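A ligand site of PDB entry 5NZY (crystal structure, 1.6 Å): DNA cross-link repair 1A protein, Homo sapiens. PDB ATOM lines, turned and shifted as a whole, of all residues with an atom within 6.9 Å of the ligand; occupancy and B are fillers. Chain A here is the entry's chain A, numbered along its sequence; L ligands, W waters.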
ATOM      1  N   ILE A 240      -4.947 -21.797 -10.020  1.00  0.00           N
ATOM      2  CA  ILE A 240      -4.626 -21.286  -8.668  1.00  0.00           C
ATOM      3  C   ILE A 240      -5.890 -21.468  -7.823  1.00  0.00           C
ATOM      4  O   ILE A 240      -6.690 -20.552  -7.604  1.00  0.00           O
ATOM      5  CB  ILE A 240      -4.123 -19.846  -8.686  1.00  0.00           C
ATOM      6  CG1 ILE A 240      -2.940 -19.716  -9.660  1.00  0.00           C
ATOM      7  CG2 ILE A 240      -3.706 -19.428  -7.272  1.00  0.00           C
ATOM      8  CD1 ILE A 240      -1.735 -20.600  -9.317  1.00  0.00           C
ATOM      9  N   ASN A 241      -6.072 -22.693  -7.351  1.00  0.00           N
ATOM     10  CA  ASN A 241      -7.162 -23.104  -6.491  1.00  0.00           C
ATOM     11  C   ASN A 241      -6.697 -24.366  -5.801  1.00  0.00           C
ATOM     12  O   ASN A 241      -5.689 -24.961  -6.194  1.00  0.00           O
ATOM     13  CB  ASN A 241      -8.468 -23.317  -7.290  1.00  0.00           C
ATOM     14  CG  ASN A 241      -8.234 -24.095  -8.580  1.00  0.00           C
ATOM     15  OD1 ASN A 241      -7.957 -25.291  -8.554  1.00  0.00           O
ATOM     16  ND2 ASN A 241      -8.355 -23.406  -9.710  1.00  0.00           N
ATOM     17  N   PHE A 242      -7.416 -24.761  -4.746  1.00  0.00           N
ATOM     18  CA  PHE A 242      -6.926 -25.856  -3.915  1.00  0.00           C
ATOM     19  C   PHE A 242      -6.751 -27.143  -4.730  1.00  0.00           C
ATOM     20  O   PHE A 242      -5.741 -27.841  -4.596  1.00  0.00           O
ATOM     21  CB  PHE A 242      -7.851 -26.084  -2.726  1.00  0.00           C
ATOM     22  CG  PHE A 242      -7.789 -24.989  -1.706  1.00  0.00           C
ATOM     23  CD1 PHE A 242      -6.570 -24.461  -1.307  1.00  0.00           C
ATOM     24  CD2 PHE A 242      -8.952 -24.485  -1.135  1.00  0.00           C
ATOM     25  CE1 PHE A 242      -6.507 -23.452  -0.360  1.00  0.00           C
ATOM     26  CE2 PHE A 242      -8.897 -23.481  -0.190  1.00  0.00           C
ATOM     27  CZ  PHE A 242      -7.681 -22.966   0.203  1.00  0.00           C
ATOM     28  N   LYS A 243      -7.719 -27.449  -5.604  1.00  0.00           N
ATOM     29  CA  LYS A 243      -7.633 -28.664  -6.402  1.00  0.00           C
ATOM     30  C   LYS A 243      -6.473 -28.583  -7.397  1.00  0.00           C
ATOM     31  O   LYS A 243      -5.695 -29.534  -7.532  1.00  0.00           O
ATOM     32  CB  LYS A 243      -8.950 -28.918  -7.142  1.00  0.00           C
ATOM     33  N   GLY A 244      -6.340 -27.458  -8.100  1.00  0.00           N
ATOM     34  CA  GLY A 244      -5.263 -27.321  -9.064  1.00  0.00           C
ATOM     35  C   GLY A 244      -3.891 -27.334  -8.417  1.00  0.00           C
ATOM     36  O   GLY A 244      -2.932 -27.863  -8.987  1.00  0.00           O
ATOM     37  N   ARG A 263      -1.967 -14.905  -6.055  1.00  0.00           N
ATOM     38  CA  ARG A 263      -2.959 -14.555  -7.067  1.00  0.00           C
ATOM     39  C   ARG A 263      -3.271 -13.069  -6.935  1.00  0.00           C
ATOM     40  O   ARG A 263      -3.600 -12.610  -5.842  1.00  0.00           O
ATOM     41  CB  ARG A 263      -4.254 -15.378  -6.902  1.00  0.00           C
ATOM     42  CG  ARG A 263      -5.429 -14.784  -7.679  1.00  0.00           C
ATOM     43  CD  ARG A 263      -6.755 -15.457  -7.344  1.00  0.00           C
ATOM     44  NE  ARG A 263      -6.918 -16.773  -7.952  1.00  0.00           N
ATOM     45  CZ  ARG A 263      -7.364 -16.972  -9.196  1.00  0.00           C
ATOM     46  NH1 ARG A 263      -7.695 -15.939  -9.956  1.00  0.00           N
ATOM     47  NH2 ARG A 263      -7.478 -18.208  -9.671  1.00  0.00           N
ATOM     48  N   PRO A 264      -3.178 -12.280  -8.011  1.00  0.00           N
ATOM     49  CA  PRO A 264      -3.538 -10.860  -7.906  1.00  0.00           C
ATOM     50  C   PRO A 264      -5.048 -10.695  -7.801  1.00  0.00           C
ATOM     51  O   PRO A 264      -5.792 -11.154  -8.672  1.00  0.00           O
ATOM     52  CB  PRO A 264      -2.995 -10.258  -9.207  1.00  0.00           C
ATOM     53  CG  PRO A 264      -1.979 -11.251  -9.696  1.00  0.00           C
ATOM     54  CD  PRO A 264      -2.523 -12.588  -9.297  1.00  0.00           C
ATOM     55  N   THR A 265      -5.500 -10.065  -6.721  1.00  0.00           N
ATOM     56  CA  THR A 265      -6.922  -9.872  -6.454  1.00  0.00           C
ATOM     57  C   THR A 265      -7.031  -8.936  -5.254  1.00  0.00           C
ATOM     58  O   THR A 265      -6.029  -8.566  -4.639  1.00  0.00           O
ATOM     59  CB  THR A 265      -7.631 -11.208  -6.177  1.00  0.00           C
ATOM     60  OG1 THR A 265      -9.040 -10.998  -6.057  1.00  0.00           O
ATOM     61  CG2 THR A 265      -7.110 -11.834  -4.899  1.00  0.00           C
ATOM     62  N   GLY A 266      -8.264  -8.542  -4.950  1.00  0.00           N
ATOM     63  CA  GLY A 266      -8.550  -7.739  -3.767  1.00  0.00           C
ATOM     64  C   GLY A 266      -8.435  -6.235  -3.974  1.00  0.00           C
ATOM     65  O   GLY A 266      -7.741  -5.550  -3.216  1.00  0.00           O
ATOM     66  N   VAL A 279      -3.565  -8.675   4.070  1.00  0.00           N
ATOM     67  CA  VAL A 279      -3.703  -9.902   3.270  1.00  0.00           C
ATOM     68  C   VAL A 279      -3.461 -11.121   4.148  1.00  0.00           C
ATOM     69  O   VAL A 279      -2.406 -11.244   4.786  1.00  0.00           O
ATOM     70  CB  VAL A 279      -2.749  -9.880   2.073  1.00  0.00           C
ATOM     71  CG1 VAL A 279      -2.635 -11.279   1.464  1.00  0.00           C
ATOM     72  CG2 VAL A 279      -3.243  -8.890   1.038  1.00  0.00           C
ATOM     73  N   ILE A 280      -4.438 -12.022   4.180  1.00  0.00           N
ATOM     74  CA  ILE A 280      -4.352 -13.297   4.898  1.00  0.00           C
ATOM     75  C   ILE A 280      -4.665 -14.413   3.907  1.00  0.00           C
ATOM     76  O   ILE A 280      -5.628 -14.285   3.133  1.00  0.00           O
ATOM     77  CB  ILE A 280      -5.300 -13.330   6.101  1.00  0.00           C
ATOM     78  CG1 ILE A 280      -5.014 -12.156   7.044  1.00  0.00           C
ATOM     79  CG2 ILE A 280      -5.213 -14.668   6.835  1.00  0.00           C
ATOM     80  CD1 ILE A 280      -3.691 -12.265   7.749  1.00  0.00           C
ATOM     81  N   PRO A 281      -3.899 -15.495   3.877  1.00  0.00           N
ATOM     82  CA  PRO A 281      -4.117 -16.520   2.855  1.00  0.00           C
ATOM     83  C   PRO A 281      -5.360 -17.365   3.117  1.00  0.00           C
ATOM     84  O   PRO A 281      -5.775 -17.549   4.260  1.00  0.00           O
ATOM     85  CB  PRO A 281      -2.849 -17.381   2.929  1.00  0.00           C
ATOM     86  CG  PRO A 281      -2.332 -17.157   4.313  1.00  0.00           C
ATOM     87  CD  PRO A 281      -2.651 -15.725   4.620  1.00  0.00           C
ATOM     88  N   GLN A 282      -5.941 -17.861   2.031  1.00  0.00           N
ATOM     89  CA  GLN A 282      -6.869 -18.982   2.112  1.00  0.00           C
ATOM     90  C   GLN A 282      -6.049 -20.260   2.199  1.00  0.00           C
ATOM     91  O   GLN A 282      -5.197 -20.504   1.338  1.00  0.00           O
ATOM     92  CB  GLN A 282      -7.799 -19.020   0.907  1.00  0.00           C
ATOM     93  CG  GLN A 282      -8.674 -17.787   0.769  1.00  0.00           C
ATOM     94  CD  GLN A 282      -9.691 -17.665   1.883  1.00  0.00           C
ATOM     95  OE1 GLN A 282     -10.168 -18.674   2.418  1.00  0.00           O
ATOM     96  NE2 GLN A 282     -10.038 -16.432   2.242  1.00  0.00           N
ATOM     97  N   THR A 283      -6.263 -21.056   3.235  1.00  0.00           N
ATOM     98  CA  THR A 283      -5.418 -22.204   3.512  1.00  0.00           C
ATOM     99  C   THR A 283      -6.258 -23.472   3.587  1.00  0.00           C
ATOM    100  O   THR A 283      -7.350 -23.461   4.157  1.00  0.00           O
ATOM    101  CB  THR A 283      -4.633 -22.005   4.824  1.00  0.00           C
ATOM    102  OG1 THR A 283      -3.799 -20.857   4.705  1.00  0.00           O
ATOM    103  CG2 THR A 283      -3.763 -23.216   5.125  1.00  0.00           C
ATOM    104  N   LYS A 284      -5.740 -24.545   2.993  1.00  0.00           N
ATOM    105  CA  LYS A 284      -6.313 -25.878   3.152  1.00  0.00           C
ATOM    106  C   LYS A 284      -5.157 -26.857   3.256  1.00  0.00           C
ATOM    107  O   LYS A 284      -4.467 -27.126   2.272  1.00  0.00           O
ATOM    108  CB  LYS A 284      -7.218 -26.240   1.972  1.00  0.00           C
ATOM    109  CG  LYS A 284      -7.874 -27.615   2.085  1.00  0.00           C
ATOM    110  CD  LYS A 284      -8.720 -27.920   0.861  1.00  0.00           C
ATOM    111  CE  LYS A 284      -9.463 -29.235   1.017  1.00  0.00           C
ATOM    112  NZ  LYS A 284     -10.470 -29.425  -0.066  1.00  0.00           N
ATOM    113  N   ILE A 289      -3.061 -19.827  -0.359  1.00  0.00           N
ATOM    114  CA  ILE A 289      -3.193 -18.933  -1.505  1.00  0.00           C
ATOM    115  C   ILE A 289      -3.314 -17.508  -0.983  1.00  0.00           C
ATOM    116  O   ILE A 289      -4.241 -17.188  -0.225  1.00  0.00           O
ATOM    117  CB  ILE A 289      -4.404 -19.299  -2.370  1.00  0.00           C
ATOM    118  CG1 ILE A 289      -4.294 -20.747  -2.836  1.00  0.00           C
ATOM    119  CG2 ILE A 289      -4.485 -18.355  -3.562  1.00  0.00           C
ATOM    120  CD1 ILE A 289      -5.534 -21.253  -3.554  1.00  0.00           C
ATOM    121  N   TYR A 290      -2.375 -16.654  -1.387  1.00  0.00           N
ATOM    122  CA  TYR A 290      -2.333 -15.246  -0.982  1.00  0.00           C
ATOM    123  C   TYR A 290      -2.928 -14.404  -2.101  1.00  0.00           C
ATOM    124  O   TYR A 290      -2.406 -14.409  -3.217  1.00  0.00           O
ATOM    125  CB  TYR A 290      -0.901 -14.797  -0.689  1.00  0.00           C
ATOM    126  CG  TYR A 290      -0.298 -15.446   0.519  1.00  0.00           C
ATOM    127  CD1 TYR A 290       0.207 -16.732   0.456  1.00  0.00           C
ATOM    128  CD2 TYR A 290      -0.238 -14.768   1.732  1.00  0.00           C
ATOM    129  CE1 TYR A 290       0.763 -17.332   1.578  1.00  0.00           C
ATOM    130  CE2 TYR A 290       0.311 -15.357   2.849  1.00  0.00           C
ATOM    131  CZ  TYR A 290       0.807 -16.640   2.766  1.00  0.00           C
ATOM    132  OH  TYR A 290       1.353 -17.238   3.868  1.00  0.00           O
ATOM    133  N   GLY A 291      -4.028 -13.711  -1.800  1.00  0.00           N
ATOM    134  CA  GLY A 291      -4.603 -12.781  -2.736  1.00  0.00           C
ATOM    135  C   GLY A 291      -3.991 -11.414  -2.551  1.00  0.00           C
ATOM    136  O   GLY A 291      -4.317 -10.709  -1.587  1.00  0.00           O
ATOM    137  N   ILE A 292      -3.079 -11.019  -3.441  1.00  0.00           N
ATOM    138  CA  ILE A 292      -2.337  -9.780  -3.236  1.00  0.00           C
ATOM    139  C   ILE A 292      -2.820  -8.714  -4.214  1.00  0.00           C
ATOM    140  O   ILE A 292      -3.040  -8.997  -5.400  1.00  0.00           O
ATOM    141  CB  ILE A 292      -0.821 -10.006  -3.347  1.00  0.00           C
ATOM    142  CG1 ILE A 292      -0.459 -10.621  -4.702  1.00  0.00           C
ATOM    143  CG2 ILE A 292      -0.341 -10.922  -2.211  1.00  0.00           C
ATOM    144  CD1 ILE A 292       1.055 -10.771  -4.910  1.00  0.00           C
HETATM  145  C1  LIG L   1      -9.796 -20.262  -2.233  1.00  0.00           C
HETATM  146  C2  LIG L   1      -9.261 -19.614  -3.424  1.00  0.00           C
HETATM  147  S1  LIG L   1     -11.235 -19.524  -1.471  1.00  0.00           S
HETATM  148  C3  LIG L   1     -11.907 -21.067  -0.839  1.00  0.00           C
HETATM  149  C4  LIG L   1     -11.967 -22.267  -1.731  1.00  0.00           C
HETATM  150  C5  LIG L   1     -11.190 -22.305  -2.846  1.00  0.00           C
HETATM  151  N1  LIG L   1     -10.255 -21.324  -3.125  1.00  0.00           N
HETATM  152  C6  LIG L   1      -9.653 -20.816  -4.208  1.00  0.00           C
HETATM  153  O1  LIG L   1      -9.598 -21.154  -5.316  1.00  0.00           O
HETATM  154  N2  LIG L   1      -9.213 -18.229  -3.637  1.00  0.00           N
HETATM  155  C7  LIG L   1      -8.557 -17.628  -4.548  1.00  0.00           C
HETATM  156  O2  LIG L   1      -7.643 -18.010  -5.234  1.00  0.00           O
HETATM  157  C8  LIG L   1      -8.866 -16.158  -4.434  1.00  0.00           C
HETATM  158  N3  LIG L   1      -8.468 -15.508  -3.421  1.00  0.00           N
HETATM  159  O3  LIG L   1      -7.674 -16.302  -2.546  1.00  0.00           O
HETATM  160  C9  LIG L   1      -6.988 -15.648  -1.471  1.00  0.00           C
HETATM  161  C10 LIG L   1      -9.618 -15.630  -5.556  1.00  0.00           C
HETATM  162  N4  LIG L   1      -9.975 -16.472  -6.562  1.00  0.00           N
HETATM  163  C11 LIG L   1     -10.626 -15.860  -7.474  1.00  0.00           C
HETATM  164  N5  LIG L   1     -11.123 -16.363  -8.580  1.00  0.00           N
HETATM  165  S2  LIG L   1     -10.743 -14.167  -7.203  1.00  0.00           S
HETATM  166  C12 LIG L   1     -10.006 -14.351  -5.702  1.00  0.00           C
HETATM  167  C13 LIG L   1     -12.977 -23.260  -1.166  1.00  0.00           C
HETATM  168  O4  LIG L   1     -12.471 -24.341  -0.285  1.00  0.00           O
HETATM  169  C14 LIG L   1     -12.646 -24.515   1.102  1.00  0.00           C
HETATM  170  O5  LIG L   1     -13.079 -25.484   1.652  1.00  0.00           O
HETATM  171  C15 LIG L   1     -12.148 -23.467   1.973  1.00  0.00           C
HETATM  172  C16 LIG L   1     -11.339 -23.397  -3.870  1.00  0.00           C
HETATM  173  O6  LIG L   1     -12.395 -23.681  -4.145  1.00  0.00           O
HETATM  174  O7  LIG L   1     -10.453 -23.851  -4.245  1.00  0.00           O
HETATM  175  O   HOH W   1      -9.384 -19.050  -7.458  1.00  0.00           O
HETATM  176  O   HOH W   2     -12.087 -14.195 -10.254  1.00  0.00           O
HETATM  177  O   HOH W   3      -5.622 -13.872   0.587  1.00  0.00           O
HETATM  178  O   HOH W   4     -12.348 -18.413 -10.717  1.00  0.00           O
HETATM  179  O   HOH W   5     -13.840 -25.852  -4.802  1.00  0.00           O
HETATM  180  O   HOH W   6     -10.449 -26.137  -5.897  1.00  0.00           O
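Residues that only touch the ligand: Asn 241, Ile 289, Gln 282, Gly 291 and Ile 240. Hydrophobic or aromatic side chains that line the ligand: Phe 242 and Ile 289. Of the 19 residues printed, 8 come within 4 Å of the ligand. Along chain A the residues within 4 Å of the ligand span positions 240 to 291.
O2 of the ligand lies within hydrogen-bond range of NE of Arg 263 (3.1 Å). O7 of the ligand sits at hydrogen-bond distance from N of Phe 242. The side-chain hydroxyl of Thr 265 lies close to a sulfur (S2) of the ligand, 3.8 Å away.
Water W1 lies within hydrogen-bond range of a nitrogen (N4) of the ligand (2.8 Å), the guanidinium group (NH2) of Arg 263 (3.0 Å) and the backbone carbonyl oxygen (O) of Ile 240 (3.1 Å). Water W6 lies within hydrogen-bond range of O7 of the ligand (2.8 Å) and N of Lys 243 (3.0 Å). Water W3 lies within hydrogen-bond range of the backbone carbonyl oxygen (O) of Ile 280 (2.6 Å) and the backbone NH (N) of Gly 291 (2.9 Å).
The backbone carbonyl oxygen (O) of Ile 240 is in hydrogen-bond range of the guanidinium group (NH2) of Arg 263 (3.2 Å). N of Arg 263 sits at hydrogen-bond distance from O of Tyr 290 (2.9 Å). N of Ile 292 lies within hydrogen-bond range of O of Arg 263, at 2.9 Å. OD1 of Asn 241 is in hydrogen-bond range of N of Gly 244, 2.7 Å away. O of Gln 282 sits at hydrogen-bond distance from N of Ile 289, 2.8 Å away. N of Thr 265 is in hydrogen-bond range of O of Ile 292, 3.0 Å away.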
